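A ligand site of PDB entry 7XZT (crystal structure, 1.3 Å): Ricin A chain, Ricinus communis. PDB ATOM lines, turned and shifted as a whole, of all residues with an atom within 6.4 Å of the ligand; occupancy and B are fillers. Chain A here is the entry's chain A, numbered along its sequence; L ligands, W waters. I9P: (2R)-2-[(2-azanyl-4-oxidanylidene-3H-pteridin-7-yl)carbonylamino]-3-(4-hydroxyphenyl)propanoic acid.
OE2 of Glu 184 lies within hydrogen-bond range of OH of Tyr 130, at 2.6 Å. The guanidinium group (NH1) of Arg 187 is in salt-bridge range of the side-chain carboxylate (OE1) of Glu 184 (3.1 Å). The side-chain amide nitrogen (ND2) of Asn 216 sits close to the backbone carbonyl oxygen (O) of Ile 212 (3.5 Å). OE1 of Glu 215 is in salt-bridge range of NH1 of Arg 141, at 2.9 Å. N of Tyr 87 sits at hydrogen-bond distance from OD1 of Asn 85 (3.0 Å). OG of Ser 183 is in hydrogen-bond range of O of Ala 86 (2.7 Å). O of Ile 179 lies within hydrogen-bond range of N of Glu 184 (3.0 Å). The backbone NH of Phe 100 is in hydrogen-bond range of the backbone carbonyl oxygen of Val 89, at 3.0 Å.
A nitrogen (N2) of the ligand lies within hydrogen-bond range of the backbone carbonyl oxygen of Gly 128. O of Val 88 is in hydrogen-bond range of N2 of the ligand, 2.8 Å away. The backbone NH (N) of Tyr 130 is in hydrogen-bond range of an oxygen (OAQ) of the ligand (2.8 Å). O4 of the ligand is in hydrogen-bond range of NH2 of Arg 187 (2.8 Å). The side-chain amide oxygen (OD1) of Asn 216 lies close to an oxygen (O) of the ligand. An oxygen (O4) of the ligand lies close to the side-chain hydroxyl of Ser 183, at 3.5 Å. The guanidinium group (NH1) of Arg 141 is in salt-bridge range of an oxygen (OXT) of the ligand (3.7 Å).
An oxygen (OXT) of the ligand sits close to the backbone carbonyl oxygen (O) of Glu 215 (3.2 Å). Ala 86 touches the ligand (O to O4, 3.5 Å). Tyr 87 touches the ligand (CE2 to C8A, 3.3 Å). CE2 of Phe 100 touches N2 of the ligand, at 3.6 Å. CA of Asn 129 touches OAQ of the ligand, at 3.5 Å. Ile 179 touches the ligand. Glu 184 touches the ligand. Hydrophobic or aromatic side chains within 4 Å of the ligand: Tyr 87, Val 88, Phe 100, Tyr 130 and Ile 179. Within 4 Å of the ligand: Ala 86, Tyr 87, Val 88, Phe 100, Gly 128, Asn 129, Tyr 130, Arg 141, Ile 179, Ser 183, Glu 184, Arg 187, Glu 215 and Asn 216. The nearest printed residue that does not touch the ligand is Asp 131 (4.7 Å).
Water W1 lies within hydrogen-bond range of an oxygen (OAQ) of the ligand (2.9 Å), the backbone NH of Asp 131 (3.0 Å) and the backbone NH of Tyr 130 (3.4 Å). Water W3 lies within hydrogen-bond range of O of Glu 215, OE2 of Glu 184 and OXT of the ligand. Water W2 bridges OH of Tyr 87 and N of the ligand.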
ATOM      1  N   ASN A  85       6.144 -24.783  32.982  1.00  0.00           N
ATOM      2  CA  ASN A  85       5.332 -23.758  32.335  1.00  0.00           C
ATOM      3  C   ASN A  85       3.986 -23.474  33.004  1.00  0.00           C
ATOM      4  O   ASN A  85       3.228 -22.631  32.522  1.00  0.00           O
ATOM      5  CB  ASN A  85       5.157 -24.093  30.845  1.00  0.00           C
ATOM      6  CG  ASN A  85       4.597 -25.489  30.623  1.00  0.00           C
ATOM      7  OD1 ASN A  85       4.042 -26.100  31.531  1.00  0.00           O
ATOM      8  ND2 ASN A  85       4.731 -25.987  29.400  1.00  0.00           N
ATOM      9  N   ALA A  86       3.708 -24.171  34.108  1.00  0.00           N
ATOM     10  CA  ALA A  86       2.410 -24.121  34.809  1.00  0.00           C
ATOM     11  C   ALA A  86       1.212 -24.644  33.975  1.00  0.00           C
ATOM     12  O   ALA A  86       0.060 -24.438  34.360  1.00  0.00           O
ATOM     13  CB  ALA A  86       2.132 -22.733  35.395  1.00  0.00           C
ATOM     14  N   TYR A  87       1.487 -25.329  32.870  1.00  0.00           N
ATOM     15  CA  TYR A  87       0.427 -25.842  31.998  1.00  0.00           C
ATOM     16  C   TYR A  87      -0.348 -26.972  32.645  1.00  0.00           C
ATOM     17  O   TYR A  87       0.234 -27.858  33.269  1.00  0.00           O
ATOM     18  CB  TYR A  87       0.971 -26.303  30.642  1.00  0.00           C
ATOM     19  CG  TYR A  87       1.031 -25.225  29.571  1.00  0.00           C
ATOM     20  CD1 TYR A  87       1.722 -24.031  29.792  1.00  0.00           C
ATOM     21  CD2 TYR A  87       0.389 -25.406  28.341  1.00  0.00           C
ATOM     22  CE1 TYR A  87       1.782 -23.047  28.822  1.00  0.00           C
ATOM     23  CE2 TYR A  87       0.450 -24.420  27.357  1.00  0.00           C
ATOM     24  CZ  TYR A  87       1.146 -23.241  27.605  1.00  0.00           C
ATOM     25  OH  TYR A  87       1.209 -22.247  26.644  1.00  0.00           O
ATOM     26  N   VAL A  88      -1.670 -26.907  32.506  1.00  0.00           N
ATOM     27  CA  VAL A  88      -2.531 -28.022  32.869  1.00  0.00           C
ATOM     28  C   VAL A  88      -2.375 -29.068  31.767  1.00  0.00           C
ATOM     29  O   VAL A  88      -2.766 -28.840  30.617  1.00  0.00           O
ATOM     30  CB  VAL A  88      -4.006 -27.587  33.018  1.00  0.00           C
ATOM     31  CG1 VAL A  88      -4.900 -28.772  33.350  1.00  0.00           C
ATOM     32  CG2 VAL A  88      -4.156 -26.500  34.083  1.00  0.00           C
ATOM     33  N   VAL A  89      -1.781 -30.206  32.113  1.00  0.00           N
ATOM     34  CA  VAL A  89      -1.497 -31.270  31.134  1.00  0.00           C
ATOM     35  C   VAL A  89      -2.587 -32.343  31.075  1.00  0.00           C
ATOM     36  O   VAL A  89      -2.655 -33.115  30.112  1.00  0.00           O
ATOM     37  CB  VAL A  89      -0.100 -31.920  31.329  1.00  0.00           C
ATOM     38  CG1 VAL A  89       1.004 -30.874  31.198  1.00  0.00           C
ATOM     39  CG2 VAL A  89       0.007 -32.659  32.659  1.00  0.00           C
ATOM     40  N   PHE A 100      -4.171 -33.970  27.624  1.00  0.00           N
ATOM     41  CA  PHE A 100      -4.084 -33.301  26.330  1.00  0.00           C
ATOM     42  C   PHE A 100      -3.022 -33.956  25.467  1.00  0.00           C
ATOM     43  O   PHE A 100      -2.082 -34.570  25.990  1.00  0.00           O
ATOM     44  CB  PHE A 100      -3.793 -31.807  26.504  1.00  0.00           C
ATOM     45  CG  PHE A 100      -4.884 -31.058  27.234  1.00  0.00           C
ATOM     46  CD1 PHE A 100      -6.171 -30.957  26.702  1.00  0.00           C
ATOM     47  CD2 PHE A 100      -4.614 -30.454  28.464  1.00  0.00           C
ATOM     48  CE1 PHE A 100      -7.174 -30.265  27.377  1.00  0.00           C
ATOM     49  CE2 PHE A 100      -5.609 -29.756  29.141  1.00  0.00           C
ATOM     50  CZ  PHE A 100      -6.886 -29.664  28.593  1.00  0.00           C
ATOM     51  N   GLY A 128      -4.037 -28.864  24.352  1.00  0.00           N
ATOM     52  CA  GLY A 128      -4.698 -28.065  25.388  1.00  0.00           C
ATOM     53  C   GLY A 128      -4.497 -26.571  25.325  1.00  0.00           C
ATOM     54  O   GLY A 128      -4.841 -25.868  26.264  1.00  0.00           O
ATOM     55  N   ASN A 129      -3.954 -26.071  24.209  1.00  0.00           N
ATOM     56  CA  ASN A 129      -3.789 -24.632  23.995  1.00  0.00           C
ATOM     57  C   ASN A 129      -5.135 -23.908  23.840  1.00  0.00           C
ATOM     58  O   ASN A 129      -6.127 -24.541  23.456  1.00  0.00           O
ATOM     59  CB  ASN A 129      -2.908 -24.382  22.759  1.00  0.00           C
ATOM     60  CG  ASN A 129      -3.394 -25.123  21.528  1.00  0.00           C
ATOM     61  OD1 ASN A 129      -3.173 -26.328  21.385  1.00  0.00           O
ATOM     62  ND2 ASN A 129      -4.074 -24.418  20.643  1.00  0.00           N
ATOM     63  N   TYR A 130      -5.149 -22.612  24.142  1.00  0.00           N
ATOM     64  CA  TYR A 130      -6.375 -21.813  24.045  1.00  0.00           C
ATOM     65  C   TYR A 130      -7.037 -21.851  22.670  1.00  0.00           C
ATOM     66  O   TYR A 130      -8.259 -22.022  22.599  1.00  0.00           O
ATOM     67  CB  TYR A 130      -6.138 -20.355  24.437  1.00  0.00           C
ATOM     68  CG  TYR A 130      -5.877 -20.090  25.905  1.00  0.00           C
ATOM     69  CD1 TYR A 130      -6.647 -20.708  26.920  1.00  0.00           C
ATOM     70  CD2 TYR A 130      -4.906 -19.181  26.289  1.00  0.00           C
ATOM     71  CE1 TYR A 130      -6.407 -20.439  28.263  1.00  0.00           C
ATOM     72  CE2 TYR A 130      -4.656 -18.904  27.621  1.00  0.00           C
ATOM     73  CZ  TYR A 130      -5.409 -19.534  28.600  1.00  0.00           C
ATOM     74  OH  TYR A 130      -5.152 -19.242  29.913  1.00  0.00           O
ATOM     75  N   ASP A 131      -6.241 -21.722  21.605  1.00  0.00           N
ATOM     76  CA  ASP A 131      -6.746 -21.757  20.222  1.00  0.00           C
ATOM     77  C   ASP A 131      -7.635 -22.970  19.964  1.00  0.00           C
ATOM     78  O   ASP A 131      -8.762 -22.832  19.474  1.00  0.00           O
ATOM     79  CB  ASP A 131      -5.589 -21.732  19.203  1.00  0.00           C
ATOM     80  CG  ASP A 131      -5.002 -20.343  18.987  1.00  0.00           C
ATOM     81  OD1 ASP A 131      -5.647 -19.326  19.323  1.00  0.00           O
ATOM     82  OD2 ASP A 131      -3.875 -20.264  18.443  1.00  0.00           O
ATOM     83  N   LEU A 133      -8.884 -25.104  22.339  1.00  0.00           N
ATOM     84  CA  LEU A 133      -9.972 -25.182  23.315  1.00  0.00           C
ATOM     85  C   LEU A 133     -11.116 -24.217  22.990  1.00  0.00           C
ATOM     86  O   LEU A 133     -12.285 -24.576  23.155  1.00  0.00           O
ATOM     87  CB  LEU A 133      -9.467 -24.981  24.755  1.00  0.00           C
ATOM     88  CG  LEU A 133      -8.554 -26.054  25.364  1.00  0.00           C
ATOM     89  CD1 LEU A 133      -8.111 -25.601  26.736  1.00  0.00           C
ATOM     90  CD2 LEU A 133      -9.213 -27.430  25.443  1.00  0.00           C
ATOM     91  N   ARG A 141     -12.132 -16.825  24.748  1.00  0.00           N
ATOM     92  CA  ARG A 141     -11.906 -16.424  26.147  1.00  0.00           C
ATOM     93  C   ARG A 141     -12.660 -15.143  26.527  1.00  0.00           C
ATOM     94  O   ARG A 141     -13.228 -15.069  27.613  1.00  0.00           O
ATOM     95  CB  ARG A 141     -10.414 -16.259  26.426  1.00  0.00           C
ATOM     96  CG  ARG A 141      -9.657 -17.547  26.703  1.00  0.00           C
ATOM     97  CD  ARG A 141      -8.156 -17.284  26.682  1.00  0.00           C
ATOM     98  NE  ARG A 141      -7.633 -17.094  25.331  1.00  0.00           N
ATOM     99  CZ  ARG A 141      -6.523 -16.439  25.019  1.00  0.00           C
ATOM    100  NH1 ARG A 141      -5.773 -15.866  25.960  1.00  0.00           N
ATOM    101  NH2 ARG A 141      -6.135 -16.355  23.754  1.00  0.00           N
ATOM    102  N   ILE A 179      -7.853 -23.209  33.644  1.00  0.00           N
ATOM    103  CA  ILE A 179      -6.528 -22.736  33.236  1.00  0.00           C
ATOM    104  C   ILE A 179      -6.319 -21.282  33.652  1.00  0.00           C
ATOM    105  O   ILE A 179      -5.267 -20.937  34.206  1.00  0.00           O
ATOM    106  CB  ILE A 179      -6.296 -22.958  31.726  1.00  0.00           C
ATOM    107  CG1 ILE A 179      -6.205 -24.457  31.401  1.00  0.00           C
ATOM    108  CG2 ILE A 179      -5.020 -22.257  31.263  1.00  0.00           C
ATOM    109  CD1 ILE A 179      -6.502 -24.809  29.964  1.00  0.00           C
ATOM    110  N   SER A 183      -3.645 -21.505  36.507  1.00  0.00           N
ATOM    111  CA  SER A 183      -2.342 -21.301  35.863  1.00  0.00           C
ATOM    112  C   SER A 183      -2.053 -19.825  35.585  1.00  0.00           C
ATOM    113  O   SER A 183      -0.979 -19.339  35.927  1.00  0.00           O
ATOM    114  CB  SER A 183      -2.227 -22.122  34.577  1.00  0.00           C
ATOM    115  OG  SER A 183      -2.451 -23.495  34.859  1.00  0.00           O
ATOM    116  N   GLU A 184      -3.009 -19.107  34.998  1.00  0.00           N
ATOM    117  CA  GLU A 184      -2.779 -17.693  34.679  1.00  0.00           C
ATOM    118  C   GLU A 184      -2.698 -16.823  35.928  1.00  0.00           C
ATOM    119  O   GLU A 184      -1.897 -15.900  35.973  1.00  0.00           O
ATOM    120  CB  GLU A 184      -3.812 -17.123  33.703  1.00  0.00           C
ATOM    121  CG  GLU A 184      -3.896 -17.843  32.370  1.00  0.00           C
ATOM    122  CD  GLU A 184      -2.709 -17.650  31.427  1.00  0.00           C
ATOM    123  OE1 GLU A 184      -1.660 -17.091  31.828  1.00  0.00           O
ATOM    124  OE2 GLU A 184      -2.835 -18.088  30.266  1.00  0.00           O
ATOM    125  N   ARG A 187       0.729 -17.294  37.251  1.00  0.00           N
ATOM    126  CA  ARG A 187       1.698 -16.567  36.433  1.00  0.00           C
ATOM    127  C   ARG A 187       1.673 -15.059  36.660  1.00  0.00           C
ATOM    128  O   ARG A 187       2.715 -14.408  36.591  1.00  0.00           O
ATOM    129  CB  ARG A 187       1.479 -16.838  34.955  1.00  0.00           C
ATOM    130  CG  ARG A 187       1.777 -18.248  34.492  1.00  0.00           C
ATOM    131  CD  ARG A 187       1.237 -18.449  33.098  1.00  0.00           C
ATOM    132  NE  ARG A 187       1.380 -19.847  32.688  1.00  0.00           N
ATOM    133  CZ  ARG A 187       0.463 -20.544  32.014  1.00  0.00           C
ATOM    134  NH1 ARG A 187      -0.688 -19.981  31.642  1.00  0.00           N
ATOM    135  NH2 ARG A 187       0.698 -21.804  31.712  1.00  0.00           N
ATOM    136  N   ILE A 212      -6.603 -10.826  28.775  1.00  0.00           N
ATOM    137  CA  ILE A 212      -6.350 -11.576  27.533  1.00  0.00           C
ATOM    138  C   ILE A 212      -4.956 -11.300  26.972  1.00  0.00           C
ATOM    139  O   ILE A 212      -4.235 -12.250  26.643  1.00  0.00           O
ATOM    140  CB  ILE A 212      -7.440 -11.292  26.458  1.00  0.00           C
ATOM    141  CG1 ILE A 212      -8.831 -11.697  26.954  1.00  0.00           C
ATOM    142  CG2 ILE A 212      -7.098 -11.975  25.124  1.00  0.00           C
ATOM    143  CD1 ILE A 212      -9.017 -13.180  27.224  1.00  0.00           C
ATOM    144  N   LEU A 214      -2.289 -10.079  28.505  1.00  0.00           N
ATOM    145  CA  LEU A 214      -1.266 -10.641  29.402  1.00  0.00           C
ATOM    146  C   LEU A 214      -1.076 -12.141  29.170  1.00  0.00           C
ATOM    147  O   LEU A 214       0.060 -12.587  28.995  1.00  0.00           O
ATOM    148  CB  LEU A 214      -1.580 -10.351  30.869  1.00  0.00           C
ATOM    149  CG  LEU A 214      -1.263  -8.963  31.412  1.00  0.00           C
ATOM    150  CD1 LEU A 214      -1.772  -8.885  32.846  1.00  0.00           C
ATOM    151  CD2 LEU A 214       0.224  -8.630  31.364  1.00  0.00           C
ATOM    152  N   GLU A 215      -2.177 -12.881  29.121  1.00  0.00           N
ATOM    153  CA  GLU A 215      -2.156 -14.318  28.819  1.00  0.00           C
ATOM    154  C   GLU A 215      -1.414 -14.600  27.519  1.00  0.00           C
ATOM    155  O   GLU A 215      -0.517 -15.436  27.464  1.00  0.00           O
ATOM    156  CB  GLU A 215      -3.576 -14.877  28.744  1.00  0.00           C
ATOM    157  CG  GLU A 215      -4.323 -14.839  30.060  1.00  0.00           C
ATOM    158  CD  GLU A 215      -5.768 -15.267  29.938  1.00  0.00           C
ATOM    159  OE1 GLU A 215      -6.251 -15.546  28.821  1.00  0.00           O
ATOM    160  OE2 GLU A 215      -6.436 -15.325  30.988  1.00  0.00           O
ATOM    161  N   ASN A 216      -1.783 -13.861  26.465  1.00  0.00           N
ATOM    162  CA  ASN A 216      -1.182 -14.032  25.150  1.00  0.00           C
ATOM    163  C   ASN A 216       0.287 -13.668  25.098  1.00  0.00           C
ATOM    164  O   ASN A 216       1.029 -14.209  24.290  1.00  0.00           O
ATOM    165  CB  ASN A 216      -1.956 -13.215  24.105  1.00  0.00           C
ATOM    166  CG  ASN A 216      -3.365 -13.745  23.855  1.00  0.00           C
ATOM    167  OD1 ASN A 216      -3.696 -14.872  24.222  1.00  0.00           O
ATOM    168  ND2 ASN A 216      -4.187 -12.933  23.215  1.00  0.00           N
ATOM    169  N   SER A 217       0.713 -12.762  25.980  1.00  0.00           N
ATOM    170  CA  SER A 217       2.068 -12.239  25.968  1.00  0.00           C
ATOM    171  C   SER A 217       3.033 -12.881  26.960  1.00  0.00           C
ATOM    172  O   SER A 217       4.192 -12.462  27.034  1.00  0.00           O
ATOM    173  CB  SER A 217       2.053 -10.723  26.183  1.00  0.00           C
ATOM    174  OG  SER A 217       1.221 -10.081  25.238  1.00  0.00           O
ATOM    175  N   TRP A 218       2.588 -13.884  27.715  1.00  0.00           N
ATOM    176  CA  TRP A 218       3.411 -14.449  28.795  1.00  0.00           C
ATOM    177  C   TRP A 218       4.785 -14.926  28.322  1.00  0.00           C
ATOM    178  O   TRP A 218       5.797 -14.595  28.926  1.00  0.00           O
ATOM    179  CB  TRP A 218       2.687 -15.577  29.528  1.00  0.00           C
ATOM    180  CG  TRP A 218       3.442 -16.103  30.728  1.00  0.00           C
ATOM    181  CD1 TRP A 218       3.859 -15.388  31.808  1.00  0.00           C
ATOM    182  CD2 TRP A 218       3.847 -17.452  30.962  1.00  0.00           C
ATOM    183  NE1 TRP A 218       4.504 -16.194  32.708  1.00  0.00           N
ATOM    184  CE2 TRP A 218       4.510 -17.482  32.218  1.00  0.00           C
ATOM    185  CE3 TRP A 218       3.717 -18.651  30.245  1.00  0.00           C
ATOM    186  CZ2 TRP A 218       5.043 -18.659  32.766  1.00  0.00           C
ATOM    187  CZ3 TRP A 218       4.240 -19.827  30.784  1.00  0.00           C
ATOM    188  CH2 TRP A 218       4.900 -19.815  32.040  1.00  0.00           C
ATOM    189  N   GLY A 219       4.808 -15.695  27.227  1.00  0.00           N
ATOM    190  CA  GLY A 219       6.060 -16.185  26.641  1.00  0.00           C
ATOM    191  C   GLY A 219       6.979 -15.061  26.215  1.00  0.00           C
ATOM    192  O   GLY A 219       8.175 -15.081  26.554  1.00  0.00           O
HETATM  193  CAL I9P L   1      -2.149 -20.876  25.632  1.00  0.00           C
HETATM  194  CG  I9P L   1       0.916 -19.881  23.485  1.00  0.00           C
HETATM  195  CB  I9P L   1       0.208 -18.652  24.066  1.00  0.00           C
HETATM  196  CA  I9P L   1      -1.262 -18.988  24.303  1.00  0.00           C
HETATM  197  C   I9P L   1      -2.115 -17.712  24.351  1.00  0.00           C
HETATM  198  OXT I9P L   1      -2.356 -17.219  25.479  1.00  0.00           O
HETATM  199  O   I9P L   1      -2.508 -17.259  23.260  1.00  0.00           O
HETATM  200  N   I9P L   1      -1.393 -19.760  25.552  1.00  0.00           N
HETATM  201  OAQ I9P L   1      -2.738 -21.348  24.664  1.00  0.00           O
HETATM  202  C7  I9P L   1      -2.141 -21.536  26.861  1.00  0.00           C
HETATM  203  N8  I9P L   1      -2.649 -22.785  26.931  1.00  0.00           N
HETATM  204  C8A I9P L   1      -2.646 -23.485  28.087  1.00  0.00           C
HETATM  205  N1  I9P L   1      -3.163 -24.718  28.100  1.00  0.00           N
HETATM  206  C2  I9P L   1      -3.193 -25.480  29.205  1.00  0.00           C
HETATM  207  N2  I9P L   1      -3.717 -26.694  29.149  1.00  0.00           N
HETATM  208  N3  I9P L   1      -2.678 -24.981  30.407  1.00  0.00           N
HETATM  209  C4  I9P L   1      -2.126 -23.702  30.428  1.00  0.00           C
HETATM  210  O4  I9P L   1      -1.678 -23.273  31.493  1.00  0.00           O
HETATM  211  C4A I9P L   1      -2.116 -22.940  29.255  1.00  0.00           C
HETATM  212  N5  I9P L   1      -1.597 -21.688  29.230  1.00  0.00           N
HETATM  213  C6  I9P L   1      -1.600 -20.966  28.020  1.00  0.00           C
HETATM  214  O   HOH W   1      -3.366 -20.892  21.828  1.00  0.00           O
HETATM  215  O   HOH W   2       1.486 -19.287  27.458  1.00  0.00           O
HETATM  216  O   HOH W   3      -0.772 -17.924  28.453  1.00  0.00           O
HETATM  217  O   HOH W   4       2.341 -16.769  25.977  1.00  0.00           O
HETATM  218  O   HOH W   5      -1.615 -27.743  26.711  1.00  0.00           O
HETATM  219  O   HOH W   6       0.555 -15.989  21.940  1.00  0.00           O
